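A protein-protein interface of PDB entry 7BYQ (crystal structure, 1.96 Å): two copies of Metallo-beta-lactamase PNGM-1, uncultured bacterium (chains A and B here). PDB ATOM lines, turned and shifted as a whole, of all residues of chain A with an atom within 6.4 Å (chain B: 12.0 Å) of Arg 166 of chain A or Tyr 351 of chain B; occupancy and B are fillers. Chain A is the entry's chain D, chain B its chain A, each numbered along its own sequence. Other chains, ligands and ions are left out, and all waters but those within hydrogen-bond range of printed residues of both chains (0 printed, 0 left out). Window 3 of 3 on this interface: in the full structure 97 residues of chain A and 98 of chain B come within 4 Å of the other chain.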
ATOM      1  N   SER A 121     -10.562  26.161  -8.806  1.00  0.00           N
ATOM      2  CA  SER A 121     -10.830  27.550  -8.361  1.00  0.00           C
ATOM      3  C   SER A 121     -10.234  27.737  -6.962  1.00  0.00           C
ATOM      4  O   SER A 121      -9.866  26.728  -6.332  1.00  0.00           O
ATOM      5  CB  SER A 121     -12.307  27.864  -8.386  1.00  0.00           C
ATOM      6  OG  SER A 121     -12.946  27.365  -7.227  1.00  0.00           O
ATOM      7  N   GLY A 122     -10.092  28.987  -6.524  1.00  0.00           N
ATOM      8  CA  GLY A 122      -9.856  29.366  -5.119  1.00  0.00           C
ATOM      9  C   GLY A 122     -11.116  29.950  -4.513  1.00  0.00           C
ATOM     10  O   GLY A 122     -12.215  29.667  -5.037  1.00  0.00           O
ATOM     11  N   ASP A 164     -14.724  23.450  -9.014  1.00  0.00           N
ATOM     12  CA  ASP A 164     -14.809  23.811  -7.571  1.00  0.00           C
ATOM     13  C   ASP A 164     -13.899  22.884  -6.762  1.00  0.00           C
ATOM     14  O   ASP A 164     -13.973  21.654  -6.968  1.00  0.00           O
ATOM     15  CB  ASP A 164     -16.244  23.717  -7.045  1.00  0.00           C
ATOM     16  CG  ASP A 164     -16.513  24.617  -5.853  1.00  0.00           C
ATOM     17  OD1 ASP A 164     -15.699  24.599  -4.898  1.00  0.00           O
ATOM     18  OD2 ASP A 164     -17.526  25.348  -5.898  1.00  0.00           O
ATOM     19  N   TYR A 165     -13.114  23.463  -5.846  1.00  0.00           N
ATOM     20  CA  TYR A 165     -12.112  22.774  -4.989  1.00  0.00           C
ATOM     21  C   TYR A 165     -12.802  22.154  -3.762  1.00  0.00           C
ATOM     22  O   TYR A 165     -12.236  21.195  -3.183  1.00  0.00           O
ATOM     23  CB  TYR A 165     -11.001  23.748  -4.585  1.00  0.00           C
ATOM     24  CG  TYR A 165     -11.418  24.836  -3.623  1.00  0.00           C
ATOM     25  CD1 TYR A 165     -12.044  25.991  -4.069  1.00  0.00           C
ATOM     26  CD2 TYR A 165     -11.185  24.714  -2.264  1.00  0.00           C
ATOM     27  CE1 TYR A 165     -12.433  26.991  -3.190  1.00  0.00           C
ATOM     28  CE2 TYR A 165     -11.559  25.706  -1.373  1.00  0.00           C
ATOM     29  CZ  TYR A 165     -12.192  26.849  -1.836  1.00  0.00           C
ATOM     30  OH  TYR A 165     -12.567  27.842  -0.975  1.00  0.00           O
ATOM     31  N   ARG A 166     -13.984  22.669  -3.393  1.00  0.00           N
ATOM     32  CA  ARG A 166     -14.788  22.231  -2.217  1.00  0.00           C
ATOM     33  C   ARG A 166     -15.745  21.091  -2.597  1.00  0.00           C
ATOM     34  O   ARG A 166     -16.512  20.660  -1.710  1.00  0.00           O
ATOM     35  CB  ARG A 166     -15.626  23.388  -1.664  1.00  0.00           C
ATOM     36  CG  ARG A 166     -14.846  24.656  -1.348  1.00  0.00           C
ATOM     37  CD  ARG A 166     -15.780  25.838  -1.122  1.00  0.00           C
ATOM     38  NE  ARG A 166     -16.607  26.112  -2.292  1.00  0.00           N
ATOM     39  CZ  ARG A 166     -17.695  26.875  -2.304  1.00  0.00           C
ATOM     40  NH1 ARG A 166     -18.122  27.468  -1.197  1.00  0.00           N
ATOM     41  NH2 ARG A 166     -18.362  27.035  -3.436  1.00  0.00           N
ATOM     42  N   ALA A 167     -15.728  20.644  -3.858  1.00  0.00           N
ATOM     43  CA  ALA A 167     -16.584  19.552  -4.385  1.00  0.00           C
ATOM     44  C   ALA A 167     -15.946  18.198  -4.055  1.00  0.00           C
ATOM     45  O   ALA A 167     -14.793  17.977  -4.478  1.00  0.00           O
ATOM     46  CB  ALA A 167     -16.791  19.727  -5.872  1.00  0.00           C
ATOM     47  N   LEU A 168     -16.686  17.337  -3.342  1.00  0.00           N
ATOM     48  CA  LEU A 168     -16.181  16.131  -2.620  1.00  0.00           C
ATOM     49  C   LEU A 168     -16.279  14.902  -3.534  1.00  0.00           C
ATOM     50  O   LEU A 168     -17.338  14.239  -3.524  1.00  0.00           O
ATOM     51  CB  LEU A 168     -17.004  15.928  -1.337  1.00  0.00           C
ATOM     52  CG  LEU A 168     -16.383  16.408  -0.023  1.00  0.00           C
ATOM     53  CD1 LEU A 168     -15.822  17.816  -0.134  1.00  0.00           C
ATOM     54  CD2 LEU A 168     -17.396  16.327   1.106  1.00  0.00           C
ATOM     55  N   TRP A 183     -11.066  15.969  -4.679  1.00  0.00           N
ATOM     56  CA  TRP A 183     -11.475  16.386  -3.315  1.00  0.00           C
ATOM     57  C   TRP A 183     -10.529  17.507  -2.903  1.00  0.00           C
ATOM     58  O   TRP A 183      -9.577  17.772  -3.630  1.00  0.00           O
ATOM     59  CB  TRP A 183     -11.500  15.187  -2.353  1.00  0.00           C
ATOM     60  CG  TRP A 183     -10.240  14.377  -2.268  1.00  0.00           C
ATOM     61  CD1 TRP A 183      -9.235  14.536  -1.360  1.00  0.00           C
ATOM     62  CD2 TRP A 183      -9.870  13.241  -3.075  1.00  0.00           C
ATOM     63  NE1 TRP A 183      -8.254  13.602  -1.567  1.00  0.00           N
ATOM     64  CE2 TRP A 183      -8.612  12.798  -2.614  1.00  0.00           C
ATOM     65  CE3 TRP A 183     -10.458  12.573  -4.154  1.00  0.00           C
ATOM     66  CZ2 TRP A 183      -7.945  11.713  -3.185  1.00  0.00           C
ATOM     67  CZ3 TRP A 183      -9.799  11.505  -4.718  1.00  0.00           C
ATOM     68  CH2 TRP A 183      -8.561  11.078  -4.238  1.00  0.00           C
ATOM     69  N   PRO A 184     -10.775  18.241  -1.794  1.00  0.00           N
ATOM     70  CA  PRO A 184      -9.893  19.338  -1.410  1.00  0.00           C
ATOM     71  C   PRO A 184      -8.538  18.805  -0.907  1.00  0.00           C
ATOM     72  O   PRO A 184      -8.264  17.635  -1.079  1.00  0.00           O
ATOM     73  CB  PRO A 184     -10.673  20.101  -0.322  1.00  0.00           C
ATOM     74  CG  PRO A 184     -12.069  19.481  -0.305  1.00  0.00           C
ATOM     75  CD  PRO A 184     -11.904  18.082  -0.862  1.00  0.00           C
ATOM     76  N   ASP A 190      -7.189  27.682   0.830  1.00  0.00           N
ATOM     77  CA  ASP A 190      -8.324  27.085   0.067  1.00  0.00           C
ATOM     78  C   ASP A 190      -7.977  27.026  -1.427  1.00  0.00           C
ATOM     79  O   ASP A 190      -7.761  28.111  -2.010  1.00  0.00           O
ATOM     80  CB  ASP A 190      -9.600  27.913   0.260  1.00  0.00           C
ATOM     81  CG  ASP A 190     -10.496  27.445   1.393  1.00  0.00           C
ATOM     82  OD1 ASP A 190     -10.000  27.316   2.531  1.00  0.00           O
ATOM     83  OD2 ASP A 190     -11.691  27.195   1.133  1.00  0.00           O
ATOM     84  N   VAL A 193      -6.306  20.642  -4.609  1.00  0.00           N
ATOM     85  CA  VAL A 193      -7.147  19.411  -4.735  1.00  0.00           C
ATOM     86  C   VAL A 193      -6.229  18.225  -5.043  1.00  0.00           C
ATOM     87  O   VAL A 193      -5.096  18.454  -5.482  1.00  0.00           O
ATOM     88  CB  VAL A 193      -8.221  19.557  -5.832  1.00  0.00           C
ATOM     89  CG1 VAL A 193      -9.296  20.566  -5.451  1.00  0.00           C
ATOM     90  CG2 VAL A 193      -7.612  19.903  -7.183  1.00  0.00           C
ATOM     91  N   TRP A 215     -10.497  13.335   3.836  1.00  0.00           N
ATOM     92  CA  TRP A 215     -10.995  13.020   2.467  1.00  0.00           C
ATOM     93  C   TRP A 215     -10.103  11.973   1.794  1.00  0.00           C
ATOM     94  O   TRP A 215     -10.642  10.925   1.399  1.00  0.00           O
ATOM     95  CB  TRP A 215     -11.103  14.266   1.580  1.00  0.00           C
ATOM     96  CG  TRP A 215     -12.042  15.318   2.074  1.00  0.00           C
ATOM     97  CD1 TRP A 215     -13.407  15.270   2.072  1.00  0.00           C
ATOM     98  CD2 TRP A 215     -11.686  16.611   2.596  1.00  0.00           C
ATOM     99  NE1 TRP A 215     -13.923  16.432   2.577  1.00  0.00           N
ATOM    100  CE2 TRP A 215     -12.894  17.278   2.897  1.00  0.00           C
ATOM    101  CE3 TRP A 215     -10.475  17.265   2.846  1.00  0.00           C
ATOM    102  CZ2 TRP A 215     -12.917  18.559   3.444  1.00  0.00           C
ATOM    103  CZ3 TRP A 215     -10.499  18.538   3.372  1.00  0.00           C
ATOM    104  CH2 TRP A 215     -11.707  19.176   3.662  1.00  0.00           C
ATOM    105  N   TRP B 142      -2.201  33.191  -6.497  1.00  0.00           N
ATOM    106  CA  TRP B 142      -2.551  32.220  -5.421  1.00  0.00           C
ATOM    107  C   TRP B 142      -1.315  31.918  -4.558  1.00  0.00           C
ATOM    108  O   TRP B 142      -1.483  31.816  -3.310  1.00  0.00           O
ATOM    109  CB  TRP B 142      -3.188  30.935  -5.972  1.00  0.00           C
ATOM    110  CG  TRP B 142      -3.570  29.960  -4.894  1.00  0.00           C
ATOM    111  CD1 TRP B 142      -4.759  29.900  -4.226  1.00  0.00           C
ATOM    112  CD2 TRP B 142      -2.749  28.918  -4.334  1.00  0.00           C
ATOM    113  NE1 TRP B 142      -4.736  28.896  -3.294  1.00  0.00           N
ATOM    114  CE2 TRP B 142      -3.517  28.274  -3.341  1.00  0.00           C
ATOM    115  CE3 TRP B 142      -1.445  28.461  -4.573  1.00  0.00           C
ATOM    116  CZ2 TRP B 142      -3.022  27.204  -2.597  1.00  0.00           C
ATOM    117  CZ3 TRP B 142      -0.958  27.404  -3.833  1.00  0.00           C
ATOM    118  CH2 TRP B 142      -1.741  26.784  -2.860  1.00  0.00           C
ATOM    119  N   SER B 346      -6.421  35.199   6.594  1.00  0.00           N
ATOM    120  CA  SER B 346      -6.161  33.823   6.113  1.00  0.00           C
ATOM    121  C   SER B 346      -6.842  33.605   4.756  1.00  0.00           C
ATOM    122  O   SER B 346      -7.939  34.161   4.535  1.00  0.00           O
ATOM    123  CB  SER B 346      -6.613  32.805   7.132  1.00  0.00           C
ATOM    124  OG  SER B 346      -6.346  31.488   6.681  1.00  0.00           O
ATOM    125  N   GLU B 347      -6.189  32.828   3.892  1.00  0.00           N
ATOM    126  CA  GLU B 347      -6.734  32.278   2.623  1.00  0.00           C
ATOM    127  C   GLU B 347      -7.329  30.888   2.879  1.00  0.00           C
ATOM    128  O   GLU B 347      -7.750  30.247   1.902  1.00  0.00           O
ATOM    129  CB  GLU B 347      -5.627  32.253   1.568  1.00  0.00           C
ATOM    130  CG  GLU B 347      -5.155  33.646   1.184  1.00  0.00           C
ATOM    131  CD  GLU B 347      -6.268  34.555   0.677  1.00  0.00           C
ATOM    132  OE1 GLU B 347      -7.250  34.032   0.122  1.00  0.00           O
ATOM    133  OE2 GLU B 347      -6.159  35.779   0.856  1.00  0.00           O
ATOM    134  N   TYR B 348      -7.333  30.439   4.143  1.00  0.00           N
ATOM    135  CA  TYR B 348      -8.142  29.293   4.638  1.00  0.00           C
ATOM    136  C   TYR B 348      -9.546  29.786   5.012  1.00  0.00           C
ATOM    137  O   TYR B 348      -9.674  30.929   5.501  1.00  0.00           O
ATOM    138  CB  TYR B 348      -7.514  28.640   5.876  1.00  0.00           C
ATOM    139  CG  TYR B 348      -6.166  28.008   5.664  1.00  0.00           C
ATOM    140  CD1 TYR B 348      -5.963  27.079   4.655  1.00  0.00           C
ATOM    141  CD2 TYR B 348      -5.091  28.320   6.486  1.00  0.00           C
ATOM    142  CE1 TYR B 348      -4.727  26.484   4.459  1.00  0.00           C
ATOM    143  CE2 TYR B 348      -3.848  27.736   6.298  1.00  0.00           C
ATOM    144  CZ  TYR B 348      -3.664  26.816   5.282  1.00  0.00           C
ATOM    145  OH  TYR B 348      -2.439  26.236   5.099  1.00  0.00           O
ATOM    146  N   THR B 349     -10.554  28.945   4.763  1.00  0.00           N
ATOM    147  CA  THR B 349     -11.926  29.015   5.332  1.00  0.00           C
ATOM    148  C   THR B 349     -12.138  27.778   6.205  1.00  0.00           C
ATOM    149  O   THR B 349     -11.534  26.739   5.877  1.00  0.00           O
ATOM    150  CB  THR B 349     -12.994  29.074   4.238  1.00  0.00           C
ATOM    151  OG1 THR B 349     -12.933  27.858   3.492  1.00  0.00           O
ATOM    152  CG2 THR B 349     -12.819  30.260   3.316  1.00  0.00           C
ATOM    153  N   GLN B 350     -12.979  27.872   7.241  1.00  0.00           N
ATOM    154  CA  GLN B 350     -13.163  26.778   8.234  1.00  0.00           C
ATOM    155  C   GLN B 350     -13.731  25.541   7.523  1.00  0.00           C
ATOM    156  O   GLN B 350     -13.566  24.435   8.065  1.00  0.00           O
ATOM    157  CB  GLN B 350     -14.021  27.239   9.416  1.00  0.00           C
ATOM    158  CG  GLN B 350     -13.936  26.323  10.632  1.00  0.00           C
ATOM    159  CD  GLN B 350     -12.575  26.255  11.283  1.00  0.00           C
ATOM    160  OE1 GLN B 350     -12.030  27.255  11.744  1.00  0.00           O
ATOM    161  NE2 GLN B 350     -12.028  25.055  11.367  1.00  0.00           N
ATOM    162  N   TYR B 351     -14.328  25.694   6.335  1.00  0.00           N
ATOM    163  CA  TYR B 351     -14.812  24.545   5.524  1.00  0.00           C
ATOM    164  C   TYR B 351     -13.657  23.571   5.224  1.00  0.00           C
ATOM    165  O   TYR B 351     -13.911  22.347   5.206  1.00  0.00           O
ATOM    166  CB  TYR B 351     -15.469  25.001   4.222  1.00  0.00           C
ATOM    167  CG  TYR B 351     -15.842  23.845   3.330  1.00  0.00           C
ATOM    168  CD1 TYR B 351     -17.025  23.151   3.514  1.00  0.00           C
ATOM    169  CD2 TYR B 351     -14.970  23.392   2.356  1.00  0.00           C
ATOM    170  CE1 TYR B 351     -17.354  22.064   2.723  1.00  0.00           C
ATOM    171  CE2 TYR B 351     -15.272  22.297   1.568  1.00  0.00           C
ATOM    172  CZ  TYR B 351     -16.471  21.635   1.745  1.00  0.00           C
ATOM    173  OH  TYR B 351     -16.768  20.563   0.959  1.00  0.00           O
ATOM    174  N   ILE B 352     -12.448  24.095   4.965  1.00  0.00           N
ATOM    175  CA  ILE B 352     -11.242  23.315   4.545  1.00  0.00           C
ATOM    176  C   ILE B 352     -10.483  22.878   5.805  1.00  0.00           C
ATOM    177  O   ILE B 352      -9.925  21.769   5.792  1.00  0.00           O
ATOM    178  CB  ILE B 352     -10.342  24.128   3.580  1.00  0.00           C
ATOM    179  CG1 ILE B 352     -10.979  24.336   2.203  1.00  0.00           C
ATOM    180  CG2 ILE B 352      -8.954  23.509   3.445  1.00  0.00           C
ATOM    181  CD1 ILE B 352     -11.218  23.067   1.406  1.00  0.00           C
ATOM    182  N   LEU B 353     -10.473  23.729   6.838  1.00  0.00           N
ATOM    183  CA  LEU B 353      -9.796  23.490   8.143  1.00  0.00           C
ATOM    184  C   LEU B 353     -10.505  22.395   8.951  1.00  0.00           C
ATOM    185  O   LEU B 353      -9.876  21.892   9.910  1.00  0.00           O
ATOM    186  CB  LEU B 353      -9.750  24.801   8.938  1.00  0.00           C
ATOM    187  CG  LEU B 353      -8.792  25.872   8.413  1.00  0.00           C
ATOM    188  CD1 LEU B 353      -8.590  26.965   9.448  1.00  0.00           C
ATOM    189  CD2 LEU B 353      -7.448  25.277   8.010  1.00  0.00           C
ATOM    190  N   ASP B 354     -11.748  22.044   8.601  1.00  0.00           N
ATOM    191  CA  ASP B 354     -12.552  21.008   9.305  1.00  0.00           C
ATOM    192  C   ASP B 354     -12.401  19.662   8.586  1.00  0.00           C
ATOM    193  O   ASP B 354     -13.169  18.741   8.907  1.00  0.00           O
ATOM    194  CB  ASP B 354     -14.015  21.443   9.440  1.00  0.00           C
ATOM    195  CG  ASP B 354     -14.224  22.634  10.364  1.00  0.00           C
ATOM    196  OD1 ASP B 354     -13.435  22.786  11.323  1.00  0.00           O
ATOM    197  OD2 ASP B 354     -15.173  23.406  10.117  1.00  0.00           O
ATOM    198  N   GLY B 355     -11.420  19.547   7.681  1.00  0.00           N
ATOM    199  CA  GLY B 355     -11.086  18.303   6.961  1.00  0.00           C
ATOM    200  C   GLY B 355      -9.795  17.661   7.447  1.00  0.00           C
ATOM    201  O   GLY B 355      -9.426  16.629   6.869  1.00  0.00           O
ATOM    202  N   ARG B 356      -9.135  18.243   8.459  1.00  0.00           N
ATOM    203  CA  ARG B 356      -7.899  17.700   9.089  1.00  0.00           C
ATOM    204  C   ARG B 356      -8.182  16.308   9.667  1.00  0.00           C
ATOM    205  O   ARG B 356      -9.326  16.064  10.086  1.00  0.00           O
ATOM    206  CB  ARG B 356      -7.391  18.614  10.210  1.00  0.00           C
ATOM    207  CG  ARG B 356      -6.630  19.841   9.737  1.00  0.00           C
ATOM    208  CD  ARG B 356      -5.909  20.519  10.884  1.00  0.00           C
ATOM    209  NE  ARG B 356      -5.235  21.743  10.478  1.00  0.00           N
ATOM    210  CZ  ARG B 356      -4.076  21.803   9.822  1.00  0.00           C
ATOM    211  NH1 ARG B 356      -3.439  20.699   9.463  1.00  0.00           N
ATOM    212  NH2 ARG B 356      -3.557  22.979   9.517  1.00  0.00           N
ATOM    213  N   LEU B 357      -7.160  15.452   9.705  1.00  0.00           N
ATOM    214  CA  LEU B 357      -7.213  14.062  10.240  1.00  0.00           C
ATOM    215  C   LEU B 357      -6.549  14.037  11.625  1.00  0.00           C
ATOM    216  O   LEU B 357      -5.540  14.747  11.797  1.00  0.00           O
ATOM    217  CB  LEU B 357      -6.490  13.156   9.236  1.00  0.00           C
ATOM    218  CG  LEU B 357      -6.390  11.671   9.583  1.00  0.00           C
ATOM    219  CD1 LEU B 357      -7.765  11.024   9.628  1.00  0.00           C
ATOM    220  CD2 LEU B 357      -5.497  10.954   8.581  1.00  0.00           C
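Printed residues of chain A that touch a printed residue of chain B: Tyr 165, Arg 166, Leu 168, Pro 184, Asp 190 and Trp 215. Hydrophobic or aromatic side chains of chain A within 4 Å of the printed part of chain B: Tyr 165, Leu 168, Pro 184 and Trp 215. Of the 13 printed residues of chain B, 7 touch a printed residue of chain A. Hydrophobic or aromatic side chains of chain B within 4 Å of the printed part of chain A: Trp 142, Tyr 351 and Ile 352. Along chain B the printed residues that touch a printed residue of chain A span positions 142 to 355. Among the printed residues, no Asp or Glu carboxylate lies within 4 Å of a Lys or Arg side-chain nitrogen of the other chain.
No residue of chain B comes within 4 Å of Ser 121 of chain A. No residue of chain B comes within 4 Å of Asp 164 of chain A. Tyr 165 of chain A touches just one residue of chain B: Ile 352. Arg 166 of chain A touches one residue of chain B. Ala 167 of chain A touches none of the printed residues of chain B. Leu 168 of chain A touches just one residue of chain B: Tyr 351. Of the printed residues of chain B, Pro 184 of chain A touches Ile 352 (3.5 Å). Printed residues of chain B within 4 Å of Trp 215 of chain A: Ile 352 (3.8 Å) and Gly 355 (3.5 Å). Printed residues of chain A within 4 Å of Trp 142 of chain B: Asp 190 (3.4 Å). Of chain A, only Arg 166 and Leu 168 come within 4 Å of Tyr 351 of chain B. Of the printed residues of chain A, Gly 355 of chain B touches Trp 215. The nearest residue of chain B that does not touch Arg 166 of chain A is Ile 352 of chain B (4.8 Å).
The side-chain carboxylate of Asp 190 of chain A is in hydrogen-bond range of the side-chain hydroxyl of Thr 349 of chain B. The backbone carbonyl oxygen (O) of Glu 347 of chain B is in hydrogen-bond range of the backbone NH (N) of Asp 190 of chain A (2.8 Å). The indole nitrogen (NE1) of Trp 142 of chain B is in hydrogen-bond range of the backbone carbonyl oxygen (O) of Asp 190 of chain A (3.4 Å). The side-chain hydroxyl (OH) of Tyr 351 of chain B lies within hydrogen-bond range of the backbone carbonyl oxygen (O) of Arg 166 of chain A (2.7 Å).
No position is printed for both chains. Of the 11 pairs that touch across the chains among the printed residues, none has its exchanged pair printed and touching as well.
Among the printed residues, pairs that only touch across the chains: Leu 168 of chain A with Tyr 351 of chain B, Asp 190 of chain A with Ile 352 of chain B, Asp 190 of chain A with Tyr 348 of chain B, Trp 215 of chain A with Gly 355 of chain B, Pro 184 of chain A with Ile 352 of chain B, Trp 215 of chain A with Ile 352 of chain B and Tyr 165 of chain A with Ile 352 of chain B.
The side-chain carboxylate (OD2) of Asp 164 of chain A lies within salt-bridge range of the guanidinium group (NH2) of Arg 166 of chain A (3.1 Å). OG of Ser 346 of chain B lies within hydrogen-bond range of N of Tyr 348 of chain B (2.9 Å).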
